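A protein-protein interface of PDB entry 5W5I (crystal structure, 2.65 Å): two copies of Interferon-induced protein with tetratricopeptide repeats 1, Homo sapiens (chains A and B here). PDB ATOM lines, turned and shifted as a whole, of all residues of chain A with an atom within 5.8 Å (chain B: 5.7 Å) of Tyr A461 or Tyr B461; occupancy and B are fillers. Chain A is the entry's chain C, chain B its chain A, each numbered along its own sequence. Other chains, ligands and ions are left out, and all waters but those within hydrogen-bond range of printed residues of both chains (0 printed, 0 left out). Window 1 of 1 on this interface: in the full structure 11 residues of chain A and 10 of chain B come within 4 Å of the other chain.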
ATOM      1  N   LEU A 441     -25.840 -34.906  12.317  1.00  0.00           N
ATOM      2  CA  LEU A 441     -25.710 -33.491  11.985  1.00  0.00           C
ATOM      3  C   LEU A 441     -25.457 -32.651  13.229  1.00  0.00           C
ATOM      4  O   LEU A 441     -24.738 -31.647  13.161  1.00  0.00           O
ATOM      5  CB  LEU A 441     -26.964 -33.001  11.259  1.00  0.00           C
ATOM      6  CG  LEU A 441     -27.194 -33.563   9.852  1.00  0.00           C
ATOM      7  CD1 LEU A 441     -28.566 -33.160   9.337  1.00  0.00           C
ATOM      8  CD2 LEU A 441     -26.109 -33.096   8.893  1.00  0.00           C
ATOM      9  N   SER A 442     -26.030 -33.044  14.369  1.00  0.00           N
ATOM     10  CA  SER A 442     -25.773 -32.329  15.615  1.00  0.00           C
ATOM     11  C   SER A 442     -24.346 -32.564  16.092  1.00  0.00           C
ATOM     12  O   SER A 442     -23.649 -31.621  16.484  1.00  0.00           O
ATOM     13  CB  SER A 442     -26.772 -32.766  16.687  1.00  0.00           C
ATOM     14  OG  SER A 442     -28.104 -32.514  16.277  1.00  0.00           O
ATOM     15  N   LEU A 443     -23.894 -33.820  16.067  1.00  0.00           N
ATOM     16  CA  LEU A 443     -22.543 -34.127  16.525  1.00  0.00           C
ATOM     17  C   LEU A 443     -21.497 -33.442  15.657  1.00  0.00           C
ATOM     18  O   LEU A 443     -20.501 -32.921  16.171  1.00  0.00           O
ATOM     19  CB  LEU A 443     -22.321 -35.640  16.541  1.00  0.00           C
ATOM     20  CG  LEU A 443     -22.515 -36.333  17.892  1.00  0.00           C
ATOM     21  CD1 LEU A 443     -23.884 -36.034  18.481  1.00  0.00           C
ATOM     22  CD2 LEU A 443     -22.326 -37.827  17.741  1.00  0.00           C
ATOM     23  N   GLY A 445     -21.867 -30.635  13.885  1.00  0.00           N
ATOM     24  CA  GLY A 445     -21.893 -29.241  14.290  1.00  0.00           C
ATOM     25  C   GLY A 445     -21.251 -29.024  15.644  1.00  0.00           C
ATOM     26  O   GLY A 445     -20.648 -27.977  15.891  1.00  0.00           O
ATOM     27  N   PHE A 446     -21.369 -30.008  16.537  1.00  0.00           N
ATOM     28  CA  PHE A 446     -20.686 -29.938  17.824  1.00  0.00           C
ATOM     29  C   PHE A 446     -19.174 -30.017  17.647  1.00  0.00           C
ATOM     30  O   PHE A 446     -18.426 -29.293  18.313  1.00  0.00           O
ATOM     31  CB  PHE A 446     -21.195 -31.059  18.728  1.00  0.00           C
ATOM     32  CG  PHE A 446     -20.452 -31.188  20.023  1.00  0.00           C
ATOM     33  CD1 PHE A 446     -20.629 -30.261  21.034  1.00  0.00           C
ATOM     34  CD2 PHE A 446     -19.593 -32.253  20.240  1.00  0.00           C
ATOM     35  CE1 PHE A 446     -19.950 -30.384  22.230  1.00  0.00           C
ATOM     36  CE2 PHE A 446     -18.916 -32.382  21.434  1.00  0.00           C
ATOM     37  CZ  PHE A 446     -19.094 -31.446  22.430  1.00  0.00           C
ATOM     38  N   VAL A 447     -18.707 -30.884  16.744  1.00  0.00           N
ATOM     39  CA  VAL A 447     -17.277 -30.972  16.456  1.00  0.00           C
ATOM     40  C   VAL A 447     -16.751 -29.627  15.965  1.00  0.00           C
ATOM     41  O   VAL A 447     -15.753 -29.107  16.476  1.00  0.00           O
ATOM     42  CB  VAL A 447     -17.006 -32.092  15.433  1.00  0.00           C
ATOM     43  CG1 VAL A 447     -15.573 -32.024  14.904  1.00  0.00           C
ATOM     44  CG2 VAL A 447     -17.267 -33.453  16.063  1.00  0.00           C
ATOM     45  N   LYS A 449     -17.850 -26.731  16.454  1.00  0.00           N
ATOM     46  CA  LYS A 449     -17.803 -25.809  17.584  1.00  0.00           C
ATOM     47  C   LYS A 449     -16.508 -25.983  18.368  1.00  0.00           C
ATOM     48  O   LYS A 449     -15.829 -25.003  18.696  1.00  0.00           O
ATOM     49  CB  LYS A 449     -19.021 -26.034  18.481  1.00  0.00           C
ATOM     50  CG  LYS A 449     -19.002 -25.261  19.791  1.00  0.00           C
ATOM     51  CD  LYS A 449     -20.167 -25.673  20.672  1.00  0.00           C
ATOM     52  CE  LYS A 449     -20.010 -25.151  22.089  1.00  0.00           C
ATOM     53  NZ  LYS A 449     -21.132 -25.591  22.965  1.00  0.00           N
ATOM     54  N   GLU A 456     -19.733 -22.747  10.758  1.00  0.00           N
ATOM     55  CA  GLU A 456     -20.136 -24.083  10.335  1.00  0.00           C
ATOM     56  C   GLU A 456     -20.906 -24.806  11.432  1.00  0.00           C
ATOM     57  O   GLU A 456     -21.786 -25.623  11.134  1.00  0.00           O
ATOM     58  CB  GLU A 456     -18.907 -24.895   9.921  1.00  0.00           C
ATOM     59  CG  GLU A 456     -18.285 -24.447   8.603  1.00  0.00           C
ATOM     60  CD  GLU A 456     -19.170 -24.752   7.403  1.00  0.00           C
ATOM     61  OE1 GLU A 456     -19.838 -25.809   7.405  1.00  0.00           O
ATOM     62  OE2 GLU A 456     -19.204 -23.933   6.459  1.00  0.00           O
ATOM     63  N   ALA A 457     -20.597 -24.521  12.698  1.00  0.00           N
ATOM     64  CA  ALA A 457     -21.361 -25.101  13.796  1.00  0.00           C
ATOM     65  C   ALA A 457     -22.815 -24.648  13.744  1.00  0.00           C
ATOM     66  O   ALA A 457     -23.737 -25.472  13.748  1.00  0.00           O
ATOM     67  CB  ALA A 457     -20.724 -24.722  15.132  1.00  0.00           C
ATOM     68  N   LEU A 458     -23.040 -23.333  13.693  1.00  0.00           N
ATOM     69  CA  LEU A 458     -24.398 -22.815  13.568  1.00  0.00           C
ATOM     70  C   LEU A 458     -25.078 -23.349  12.314  1.00  0.00           C
ATOM     71  O   LEU A 458     -26.277 -23.652  12.329  1.00  0.00           O
ATOM     72  CB  LEU A 458     -24.375 -21.286  13.547  1.00  0.00           C
ATOM     73  CG  LEU A 458     -23.870 -20.598  14.816  1.00  0.00           C
ATOM     74  CD1 LEU A 458     -23.612 -19.123  14.556  1.00  0.00           C
ATOM     75  CD2 LEU A 458     -24.865 -20.771  15.952  1.00  0.00           C
ATOM     76  N   GLU A 459     -24.329 -23.474  11.217  1.00  0.00           N
ATOM     77  CA  GLU A 459     -24.921 -23.944   9.970  1.00  0.00           C
ATOM     78  C   GLU A 459     -25.463 -25.361  10.115  1.00  0.00           C
ATOM     79  O   GLU A 459     -26.552 -25.669   9.617  1.00  0.00           O
ATOM     80  CB  GLU A 459     -23.891 -23.871   8.841  1.00  0.00           C
ATOM     81  CG  GLU A 459     -24.334 -23.026   7.655  1.00  0.00           C
ATOM     82  CD  GLU A 459     -23.198 -22.721   6.695  1.00  0.00           C
ATOM     83  OE1 GLU A 459     -22.243 -22.025   7.103  1.00  0.00           O
ATOM     84  OE2 GLU A 459     -23.255 -23.182   5.534  1.00  0.00           O
ATOM     85  N   TYR A 460     -24.724 -26.236  10.802  1.00  0.00           N
ATOM     86  CA  TYR A 460     -25.179 -27.612  10.977  1.00  0.00           C
ATOM     87  C   TYR A 460     -26.232 -27.725  12.073  1.00  0.00           C
ATOM     88  O   TYR A 460     -27.183 -28.504  11.940  1.00  0.00           O
ATOM     89  CB  TYR A 460     -23.994 -28.526  11.278  1.00  0.00           C
ATOM     90  CG  TYR A 460     -23.273 -29.000  10.038  1.00  0.00           C
ATOM     91  CD1 TYR A 460     -22.154 -28.332   9.562  1.00  0.00           C
ATOM     92  CD2 TYR A 460     -23.720 -30.113   9.337  1.00  0.00           C
ATOM     93  CE1 TYR A 460     -21.497 -28.760   8.425  1.00  0.00           C
ATOM     94  CE2 TYR A 460     -23.070 -30.548   8.198  1.00  0.00           C
ATOM     95  CZ  TYR A 460     -21.958 -29.868   7.746  1.00  0.00           C
ATOM     96  OH  TYR A 460     -21.306 -30.297   6.614  1.00  0.00           O
ATOM     97  N   TYR A 461     -26.082 -26.970  13.163  1.00  0.00           N
ATOM     98  CA  TYR A 461     -27.120 -26.945  14.189  1.00  0.00           C
ATOM     99  C   TYR A 461     -28.452 -26.503  13.596  1.00  0.00           C
ATOM    100  O   TYR A 461     -29.495 -27.116  13.850  1.00  0.00           O
ATOM    101  CB  TYR A 461     -26.713 -26.015  15.335  1.00  0.00           C
ATOM    102  CG  TYR A 461     -25.735 -26.597  16.343  1.00  0.00           C
ATOM    103  CD1 TYR A 461     -25.414 -27.950  16.351  1.00  0.00           C
ATOM    104  CD2 TYR A 461     -25.142 -25.782  17.301  1.00  0.00           C
ATOM    105  CE1 TYR A 461     -24.530 -28.469  17.275  1.00  0.00           C
ATOM    106  CE2 TYR A 461     -24.257 -26.293  18.227  1.00  0.00           C
ATOM    107  CZ  TYR A 461     -23.954 -27.637  18.211  1.00  0.00           C
ATOM    108  OH  TYR A 461     -23.071 -28.153  19.133  1.00  0.00           O
ATOM    109  N   GLU A 462     -28.435 -25.433  12.800  1.00  0.00           N
ATOM    110  CA  GLU A 462     -29.657 -24.980  12.147  1.00  0.00           C
ATOM    111  C   GLU A 462     -30.187 -26.040  11.192  1.00  0.00           C
ATOM    112  O   GLU A 462     -31.385 -26.347  11.193  1.00  0.00           O
ATOM    113  CB  GLU A 462     -29.399 -23.666  11.411  1.00  0.00           C
ATOM    114  CG  GLU A 462     -29.150 -22.494  12.339  1.00  0.00           C
ATOM    115  CD  GLU A 462     -28.749 -21.239  11.600  1.00  0.00           C
ATOM    116  OE1 GLU A 462     -28.592 -21.299  10.361  1.00  0.00           O
ATOM    117  OE2 GLU A 462     -28.591 -20.190  12.258  1.00  0.00           O
ATOM    118  N   ARG A 463     -29.306 -26.616  10.370  1.00  0.00           N
ATOM    119  CA  ARG A 463     -29.737 -27.666   9.452  1.00  0.00           C
ATOM    120  C   ARG A 463     -30.385 -28.818  10.209  1.00  0.00           C
ATOM    121  O   ARG A 463     -31.353 -29.420   9.731  1.00  0.00           O
ATOM    122  CB  ARG A 463     -28.555 -28.169   8.625  1.00  0.00           C
ATOM    123  CG  ARG A 463     -28.978 -28.951   7.386  1.00  0.00           C
ATOM    124  CD  ARG A 463     -27.874 -29.858   6.859  1.00  0.00           C
ATOM    125  NE  ARG A 463     -26.738 -29.118   6.318  1.00  0.00           N
ATOM    126  CZ  ARG A 463     -25.757 -29.671   5.610  1.00  0.00           C
ATOM    127  NH1 ARG A 463     -25.770 -30.972   5.348  1.00  0.00           N
ATOM    128  NH2 ARG A 463     -24.760 -28.922   5.159  1.00  0.00           N
ATOM    129  N   ALA A 464     -29.866 -29.137  11.396  1.00  0.00           N
ATOM    130  CA  ALA A 464     -30.440 -30.218  12.188  1.00  0.00           C
ATOM    131  C   ALA A 464     -31.782 -29.813  12.787  1.00  0.00           C
ATOM    132  O   ALA A 464     -32.735 -30.601  12.777  1.00  0.00           O
ATOM    133  CB  ALA A 464     -29.466 -30.634  13.290  1.00  0.00           C
ATOM    134  N   LEU A 465     -31.879 -28.589  13.313  1.00  0.00           N
ATOM    135  CA  LEU A 465     -33.126 -28.134  13.916  1.00  0.00           C
ATOM    136  C   LEU A 465     -34.266 -28.064  12.908  1.00  0.00           C
ATOM    137  O   LEU A 465     -35.434 -28.081  13.310  1.00  0.00           O
ATOM    138  CB  LEU A 465     -32.924 -26.767  14.572  1.00  0.00           C
ATOM    139  CG  LEU A 465     -32.203 -26.787  15.924  1.00  0.00           C
ATOM    140  CD1 LEU A 465     -31.758 -25.390  16.320  1.00  0.00           C
ATOM    141  CD2 LEU A 465     -33.096 -27.380  17.002  1.00  0.00           C
ATOM    142  N   ARG A 466     -33.959 -27.983  11.610  1.00  0.00           N
ATOM    143  CA  ARG A 466     -35.015 -28.046  10.606  1.00  0.00           C
ATOM    144  C   ARG A 466     -35.579 -29.457  10.495  1.00  0.00           C
ATOM    145  O   ARG A 466     -36.798 -29.638  10.394  1.00  0.00           O
ATOM    146  CB  ARG A 466     -34.486 -27.569   9.252  1.00  0.00           C
ATOM    147  CG  ARG A 466     -34.076 -26.102   9.232  1.00  0.00           C
ATOM    148  CD  ARG A 466     -33.973 -25.558   7.813  1.00  0.00           C
ATOM    149  NE  ARG A 466     -32.619 -25.121   7.477  1.00  0.00           N
ATOM    150  CZ  ARG A 466     -31.712 -25.865   6.846  1.00  0.00           C
ATOM    151  NH1 ARG A 466     -31.994 -27.105   6.467  1.00  0.00           N
ATOM    152  NH2 ARG A 466     -30.510 -25.363   6.591  1.00  0.00           N
ATOM    153  N   LEU B 441     -37.218 -22.244  21.583  1.00  0.00           N
ATOM    154  CA  LEU B 441     -35.790 -22.352  21.858  1.00  0.00           C
ATOM    155  C   LEU B 441     -34.968 -22.075  20.606  1.00  0.00           C
ATOM    156  O   LEU B 441     -33.941 -21.388  20.672  1.00  0.00           O
ATOM    157  CB  LEU B 441     -35.463 -23.737  22.414  1.00  0.00           C
ATOM    158  CG  LEU B 441     -35.950 -24.033  23.833  1.00  0.00           C
ATOM    159  CD1 LEU B 441     -35.798 -25.513  24.141  1.00  0.00           C
ATOM    160  CD2 LEU B 441     -35.189 -23.195  24.851  1.00  0.00           C
ATOM    161  N   SER B 442     -35.405 -22.594  19.457  1.00  0.00           N
ATOM    162  CA  SER B 442     -34.675 -22.361  18.216  1.00  0.00           C
ATOM    163  C   SER B 442     -34.704 -20.887  17.830  1.00  0.00           C
ATOM    164  O   SER B 442     -33.679 -20.325  17.430  1.00  0.00           O
ATOM    165  CB  SER B 442     -35.261 -23.218  17.096  1.00  0.00           C
ATOM    166  OG  SER B 442     -35.298 -24.583  17.468  1.00  0.00           O
ATOM    167  N   LEU B 443     -35.870 -20.246  17.946  1.00  0.00           N
ATOM    168  CA  LEU B 443     -35.981 -18.841  17.572  1.00  0.00           C
ATOM    169  C   LEU B 443     -35.133 -17.956  18.478  1.00  0.00           C
ATOM    170  O   LEU B 443     -34.525 -16.986  18.012  1.00  0.00           O
ATOM    171  CB  LEU B 443     -37.446 -18.403  17.611  1.00  0.00           C
ATOM    172  CG  LEU B 443     -38.321 -18.911  16.464  1.00  0.00           C
ATOM    173  CD1 LEU B 443     -39.783 -18.651  16.765  1.00  0.00           C
ATOM    174  CD2 LEU B 443     -37.927 -18.257  15.147  1.00  0.00           C
ATOM    175  N   GLY B 445     -32.355 -18.822  19.944  1.00  0.00           N
ATOM    176  CA  GLY B 445     -30.982 -18.984  19.497  1.00  0.00           C
ATOM    177  C   GLY B 445     -30.722 -18.261  18.190  1.00  0.00           C
ATOM    178  O   GLY B 445     -29.647 -17.691  17.987  1.00  0.00           O
ATOM    179  N   PHE B 446     -31.704 -18.276  17.286  1.00  0.00           N
ATOM    180  CA  PHE B 446     -31.598 -17.505  16.052  1.00  0.00           C
ATOM    181  C   PHE B 446     -31.507 -16.014  16.346  1.00  0.00           C
ATOM    182  O   PHE B 446     -30.777 -15.281  15.669  1.00  0.00           O
ATOM    183  CB  PHE B 446     -32.797 -17.812  15.154  1.00  0.00           C
ATOM    184  CG  PHE B 446     -32.819 -17.033  13.871  1.00  0.00           C
ATOM    185  CD1 PHE B 446     -31.926 -17.321  12.855  1.00  0.00           C
ATOM    186  CD2 PHE B 446     -33.748 -16.026  13.674  1.00  0.00           C
ATOM    187  CE1 PHE B 446     -31.952 -16.610  11.669  1.00  0.00           C
ATOM    188  CE2 PHE B 446     -33.780 -15.314  12.492  1.00  0.00           C
ATOM    189  CZ  PHE B 446     -32.881 -15.605  11.489  1.00  0.00           C
ATOM    190  N   VAL B 447     -32.241 -15.548  17.359  1.00  0.00           N
ATOM    191  CA  VAL B 447     -32.191 -14.138  17.740  1.00  0.00           C
ATOM    192  C   VAL B 447     -30.797 -13.773  18.234  1.00  0.00           C
ATOM    193  O   VAL B 447     -30.217 -12.761  17.822  1.00  0.00           O
ATOM    194  CB  VAL B 447     -33.268 -13.835  18.798  1.00  0.00           C
ATOM    195  CG1 VAL B 447     -32.967 -12.539  19.546  1.00  0.00           C
ATOM    196  CG2 VAL B 447     -34.640 -13.755  18.141  1.00  0.00           C
ATOM    197  N   LYS B 449     -28.027 -15.106  17.548  1.00  0.00           N
ATOM    198  CA  LYS B 449     -27.086 -15.073  16.433  1.00  0.00           C
ATOM    199  C   LYS B 449     -27.118 -13.715  15.741  1.00  0.00           C
ATOM    200  O   LYS B 449     -26.071 -13.114  15.476  1.00  0.00           O
ATOM    201  CB  LYS B 449     -27.404 -16.189  15.437  1.00  0.00           C
ATOM    202  CG  LYS B 449     -26.410 -16.276  14.286  1.00  0.00           C
ATOM    203  CD  LYS B 449     -26.737 -17.397  13.313  1.00  0.00           C
ATOM    204  CE  LYS B 449     -27.840 -17.000  12.346  1.00  0.00           C
ATOM    205  NZ  LYS B 449     -27.943 -17.949  11.202  1.00  0.00           N
ATOM    206  N   GLU B 456     -24.421 -17.686  23.249  1.00  0.00           N
ATOM    207  CA  GLU B 456     -25.807 -17.934  23.630  1.00  0.00           C
ATOM    208  C   GLU B 456     -26.574 -18.605  22.498  1.00  0.00           C
ATOM    209  O   GLU B 456     -27.452 -19.442  22.743  1.00  0.00           O
ATOM    210  CB  GLU B 456     -26.486 -16.623  24.030  1.00  0.00           C
ATOM    211  CG  GLU B 456     -26.022 -16.055  25.362  1.00  0.00           C
ATOM    212  CD  GLU B 456     -26.412 -16.932  26.538  1.00  0.00           C
ATOM    213  OE1 GLU B 456     -25.757 -17.975  26.752  1.00  0.00           O
ATOM    214  OE2 GLU B 456     -27.383 -16.584  27.243  1.00  0.00           O
ATOM    215  N   ALA B 457     -26.260 -18.252  21.250  1.00  0.00           N
ATOM    216  CA  ALA B 457     -26.920 -18.888  20.114  1.00  0.00           C
ATOM    217  C   ALA B 457     -26.601 -20.378  20.068  1.00  0.00           C
ATOM    218  O   ALA B 457     -27.502 -21.215  19.931  1.00  0.00           O
ATOM    219  CB  ALA B 457     -26.499 -18.204  18.813  1.00  0.00           C
ATOM    220  N   LEU B 458     -25.320 -20.729  20.185  1.00  0.00           N
ATOM    221  CA  LEU B 458     -24.941 -22.138  20.224  1.00  0.00           C
ATOM    222  C   LEU B 458     -25.592 -22.844  21.405  1.00  0.00           C
ATOM    223  O   LEU B 458     -25.967 -24.019  21.306  1.00  0.00           O
ATOM    224  CB  LEU B 458     -23.419 -22.271  20.292  1.00  0.00           C
ATOM    225  CG  LEU B 458     -22.642 -21.878  19.035  1.00  0.00           C
ATOM    226  CD1 LEU B 458     -21.158 -21.796  19.335  1.00  0.00           C
ATOM    227  CD2 LEU B 458     -22.900 -22.870  17.913  1.00  0.00           C
ATOM    228  N   GLU B 459     -25.738 -22.147  22.531  1.00  0.00           N
ATOM    229  CA  GLU B 459     -26.353 -22.751  23.707  1.00  0.00           C
ATOM    230  C   GLU B 459     -27.798 -23.147  23.420  1.00  0.00           C
ATOM    231  O   GLU B 459     -28.149 -24.331  23.446  1.00  0.00           O
ATOM    232  CB  GLU B 459     -26.278 -21.784  24.891  1.00  0.00           C
ATOM    233  CG  GLU B 459     -26.750 -22.383  26.209  1.00  0.00           C
ATOM    234  CD  GLU B 459     -26.595 -21.425  27.377  1.00  0.00           C
ATOM    235  OE1 GLU B 459     -25.730 -20.526  27.305  1.00  0.00           O
ATOM    236  OE2 GLU B 459     -27.343 -21.571  28.368  1.00  0.00           O
ATOM    237  N   TYR B 460     -28.650 -22.162  23.123  1.00  0.00           N
ATOM    238  CA  TYR B 460     -30.069 -22.444  22.932  1.00  0.00           C
ATOM    239  C   TYR B 460     -30.312 -23.356  21.736  1.00  0.00           C
ATOM    240  O   TYR B 460     -31.310 -24.085  21.709  1.00  0.00           O
ATOM    241  CB  TYR B 460     -30.847 -21.137  22.784  1.00  0.00           C
ATOM    242  CG  TYR B 460     -31.109 -20.458  24.109  1.00  0.00           C
ATOM    243  CD1 TYR B 460     -30.288 -19.436  24.565  1.00  0.00           C
ATOM    244  CD2 TYR B 460     -32.169 -20.855  24.916  1.00  0.00           C
ATOM    245  CE1 TYR B 460     -30.521 -18.820  25.781  1.00  0.00           C
ATOM    246  CE2 TYR B 460     -32.407 -20.248  26.136  1.00  0.00           C
ATOM    247  CZ  TYR B 460     -31.581 -19.228  26.562  1.00  0.00           C
ATOM    248  OH  TYR B 460     -31.815 -18.618  27.773  1.00  0.00           O
ATOM    249  N   TYR B 461     -29.423 -23.335  20.740  1.00  0.00           N
ATOM    250  CA  TYR B 461     -29.516 -24.310  19.658  1.00  0.00           C
ATOM    251  C   TYR B 461     -29.245 -25.719  20.173  1.00  0.00           C
ATOM    252  O   TYR B 461     -29.876 -26.683  19.724  1.00  0.00           O
ATOM    253  CB  TYR B 461     -28.534 -23.964  18.536  1.00  0.00           C
ATOM    254  CG  TYR B 461     -29.005 -22.929  17.530  1.00  0.00           C
ATOM    255  CD1 TYR B 461     -30.293 -22.401  17.574  1.00  0.00           C
ATOM    256  CD2 TYR B 461     -28.156 -22.488  16.523  1.00  0.00           C
ATOM    257  CE1 TYR B 461     -30.712 -21.462  16.648  1.00  0.00           C
ATOM    258  CE2 TYR B 461     -28.567 -21.550  15.595  1.00  0.00           C
ATOM    259  CZ  TYR B 461     -29.845 -21.040  15.663  1.00  0.00           C
ATOM    260  OH  TYR B 461     -30.256 -20.107  14.740  1.00  0.00           O
ATOM    261  N   GLU B 462     -28.313 -25.857  21.117  1.00  0.00           N
ATOM    262  CA  GLU B 462     -27.960 -27.178  21.622  1.00  0.00           C
ATOM    263  C   GLU B 462     -29.044 -27.721  22.543  1.00  0.00           C
ATOM    264  O   GLU B 462     -29.537 -28.837  22.342  1.00  0.00           O
ATOM    265  CB  GLU B 462     -26.613 -27.118  22.339  1.00  0.00           C
ATOM    266  CG  GLU B 462     -25.426 -27.028  21.391  1.00  0.00           C
ATOM    267  CD  GLU B 462     -24.115 -26.789  22.112  1.00  0.00           C
ATOM    268  OE1 GLU B 462     -24.137 -26.592  23.346  1.00  0.00           O
ATOM    269  OE2 GLU B 462     -23.061 -26.797  21.442  1.00  0.00           O
ATOM    270  N   ARG B 463     -29.436 -26.948  23.559  1.00  0.00           N
ATOM    271  CA  ARG B 463     -30.489 -27.404  24.459  1.00  0.00           C
ATOM    272  C   ARG B 463     -31.830 -27.551  23.755  1.00  0.00           C
ATOM    273  O   ARG B 463     -32.748 -28.145  24.331  1.00  0.00           O
ATOM    274  CB  ARG B 463     -30.627 -26.458  25.658  1.00  0.00           C
ATOM    275  CG  ARG B 463     -30.743 -24.991  25.321  1.00  0.00           C
ATOM    276  CD  ARG B 463     -30.853 -24.156  26.586  1.00  0.00           C
ATOM    277  NE  ARG B 463     -32.125 -24.373  27.268  1.00  0.00           N
ATOM    278  CZ  ARG B 463     -32.440 -23.854  28.450  1.00  0.00           C
ATOM    279  NH1 ARG B 463     -31.572 -23.084  29.096  1.00  0.00           N
ATOM    280  NH2 ARG B 463     -33.625 -24.107  28.989  1.00  0.00           N
ATOM    281  N   ALA B 464     -31.967 -27.032  22.534  1.00  0.00           N
ATOM    282  CA  ALA B 464     -33.148 -27.316  21.727  1.00  0.00           C
ATOM    283  C   ALA B 464     -32.997 -28.635  20.980  1.00  0.00           C
ATOM    284  O   ALA B 464     -33.970 -29.383  20.832  1.00  0.00           O
ATOM    285  CB  ALA B 464     -33.401 -26.178  20.737  1.00  0.00           C
ATOM    286  N   LEU B 465     -31.787 -28.932  20.501  1.00  0.00           N
ATOM    287  CA  LEU B 465     -31.527 -30.210  19.852  1.00  0.00           C
ATOM    288  C   LEU B 465     -31.645 -31.380  20.820  1.00  0.00           C
ATOM    289  O   LEU B 465     -31.822 -32.519  20.375  1.00  0.00           O
ATOM    290  CB  LEU B 465     -30.137 -30.204  19.213  1.00  0.00           C
ATOM    291  CG  LEU B 465     -29.998 -29.386  17.927  1.00  0.00           C
ATOM    292  CD1 LEU B 465     -28.532 -29.177  17.577  1.00  0.00           C
ATOM    293  CD2 LEU B 465     -30.726 -30.066  16.776  1.00  0.00           C
ATOM    294  N   ARG B 466     -31.548 -31.131  22.127  1.00  0.00           N
ATOM    295  CA  ARG B 466     -31.770 -32.202  23.092  1.00  0.00           C
ATOM    296  C   ARG B 466     -33.245 -32.574  23.153  1.00  0.00           C
ATOM    297  O   ARG B 466     -33.591 -33.761  23.182  1.00  0.00           O
ATOM    298  CB  ARG B 466     -31.254 -31.787  24.469  1.00  0.00           C
ATOM    299  CG  ARG B 466     -29.786 -31.393  24.461  1.00  0.00           C
ATOM    300  CD  ARG B 466     -29.217 -31.235  25.858  1.00  0.00           C
ATOM    301  NE  ARG B 466     -27.990 -30.438  25.834  1.00  0.00           N
ATOM    302  CZ  ARG B 466     -27.845 -29.234  26.384  1.00  0.00           C
ATOM    303  NH1 ARG B 466     -28.842 -28.656  27.042  1.00  0.00           N
ATOM    304  NH2 ARG B 466     -26.681 -28.605  26.289  1.00  0.00           N
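The side-chain carboxylate of Glu A462 is in salt-bridge range of the side-chain amino group of Lys B449 (2.6 Å).
OH of Tyr B461 lies within hydrogen-bond range of OE2 of Glu A462 (3.0 Å).
OE2 of Glu B462 lies within salt-bridge range of NZ of Lys A449.
The side-chain carboxylate (OE2) of Glu B462 lies within hydrogen-bond range of the side-chain hydroxyl (OH) of Tyr A461 (2.7 Å).
The backbone NH (N) of Phe B446 sits close to the side-chain hydroxyl (OH) of Tyr B461 (3.5 Å).
Ser A442 touches Leu B465 (OG to CD1, 3.6 Å).
Ala A457 touches Leu B458.
Leu A458 touches Lys B449.
Leu B458 touches Leu A458 (CD2 to CD2, 3.5 Å).
Leu A458 touches Tyr B461 (CD2 to CD2, 3.8 Å).
CE2 of Tyr A461 touches CD2 of Leu B458, at 3.7 Å.
CB of Tyr A461 touches CD2 of Tyr B461 (3.99 Å).
Tyr B461 touches Leu A465 (CD1 to CD1, 3.6 Å).
CD2 of Leu A465 touches CB of Ala B464 (3.9 Å).
Leu A465 touches Leu B465.
Of the printed residues of chain B, Tyr A461 touches Leu B458, Tyr B461, Glu B462 and Leu B465.
Of the printed residues of chain B, Ala A464 touches Leu B465 (3.7 Å).
Printed residues of chain B within 4 Å of Lys A449: Glu B462.
Leu B443 touches none of the printed residues of chain A.
The nearest printed residue of chain B that does not touch Tyr A461 is Ala B457 (5.8 Å).
The nearest printed residue of chain A that does not touch Glu B462 is Phe A446 (4.3 Å).
Hydrophobic or aromatic side chains of chain A within 4 Å of the printed part of chain B: Ala A457, Leu A458, Tyr A461, Ala A464 and Leu A465.
Along chain A the printed residues that touch a printed residue of chain B span positions 442 to 465.
Of the 18 printed residues of chain B, 7 touch a printed residue of chain A.
Among the printed residues, 17 pairs touch across the chains.
Among the printed residues, Asp or Glu carboxylates within 4 Å of a Lys or Arg side-chain nitrogen of the other chain: Lys A449 with Glu B462 and Glu A462 with Lys B449.
Ala A457 touches Leu B458, but with the chains exchanged Leu A458 does not touch Ala B457 (4.2 Å).
Leu A458 touches Tyr B461, and with the chains exchanged Tyr A461 touches Leu B458.
Tyr A461 touches Glu B462, and with the chains exchanged Glu A462 touches Tyr B461.
Ala A464 touches Leu B465, and with the chains exchanged Leu A465 touches Ala B464.
Positions printed for both chains: 441, 442, 443, 445, 446, 447, 449, 456, 457, 458, 459, 460, 461, 462, 463, 464, 465 and 466.
Of the 17 pairs that touch across the chains among the printed residues, 15 have their exchanged pair printed and touching as well.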
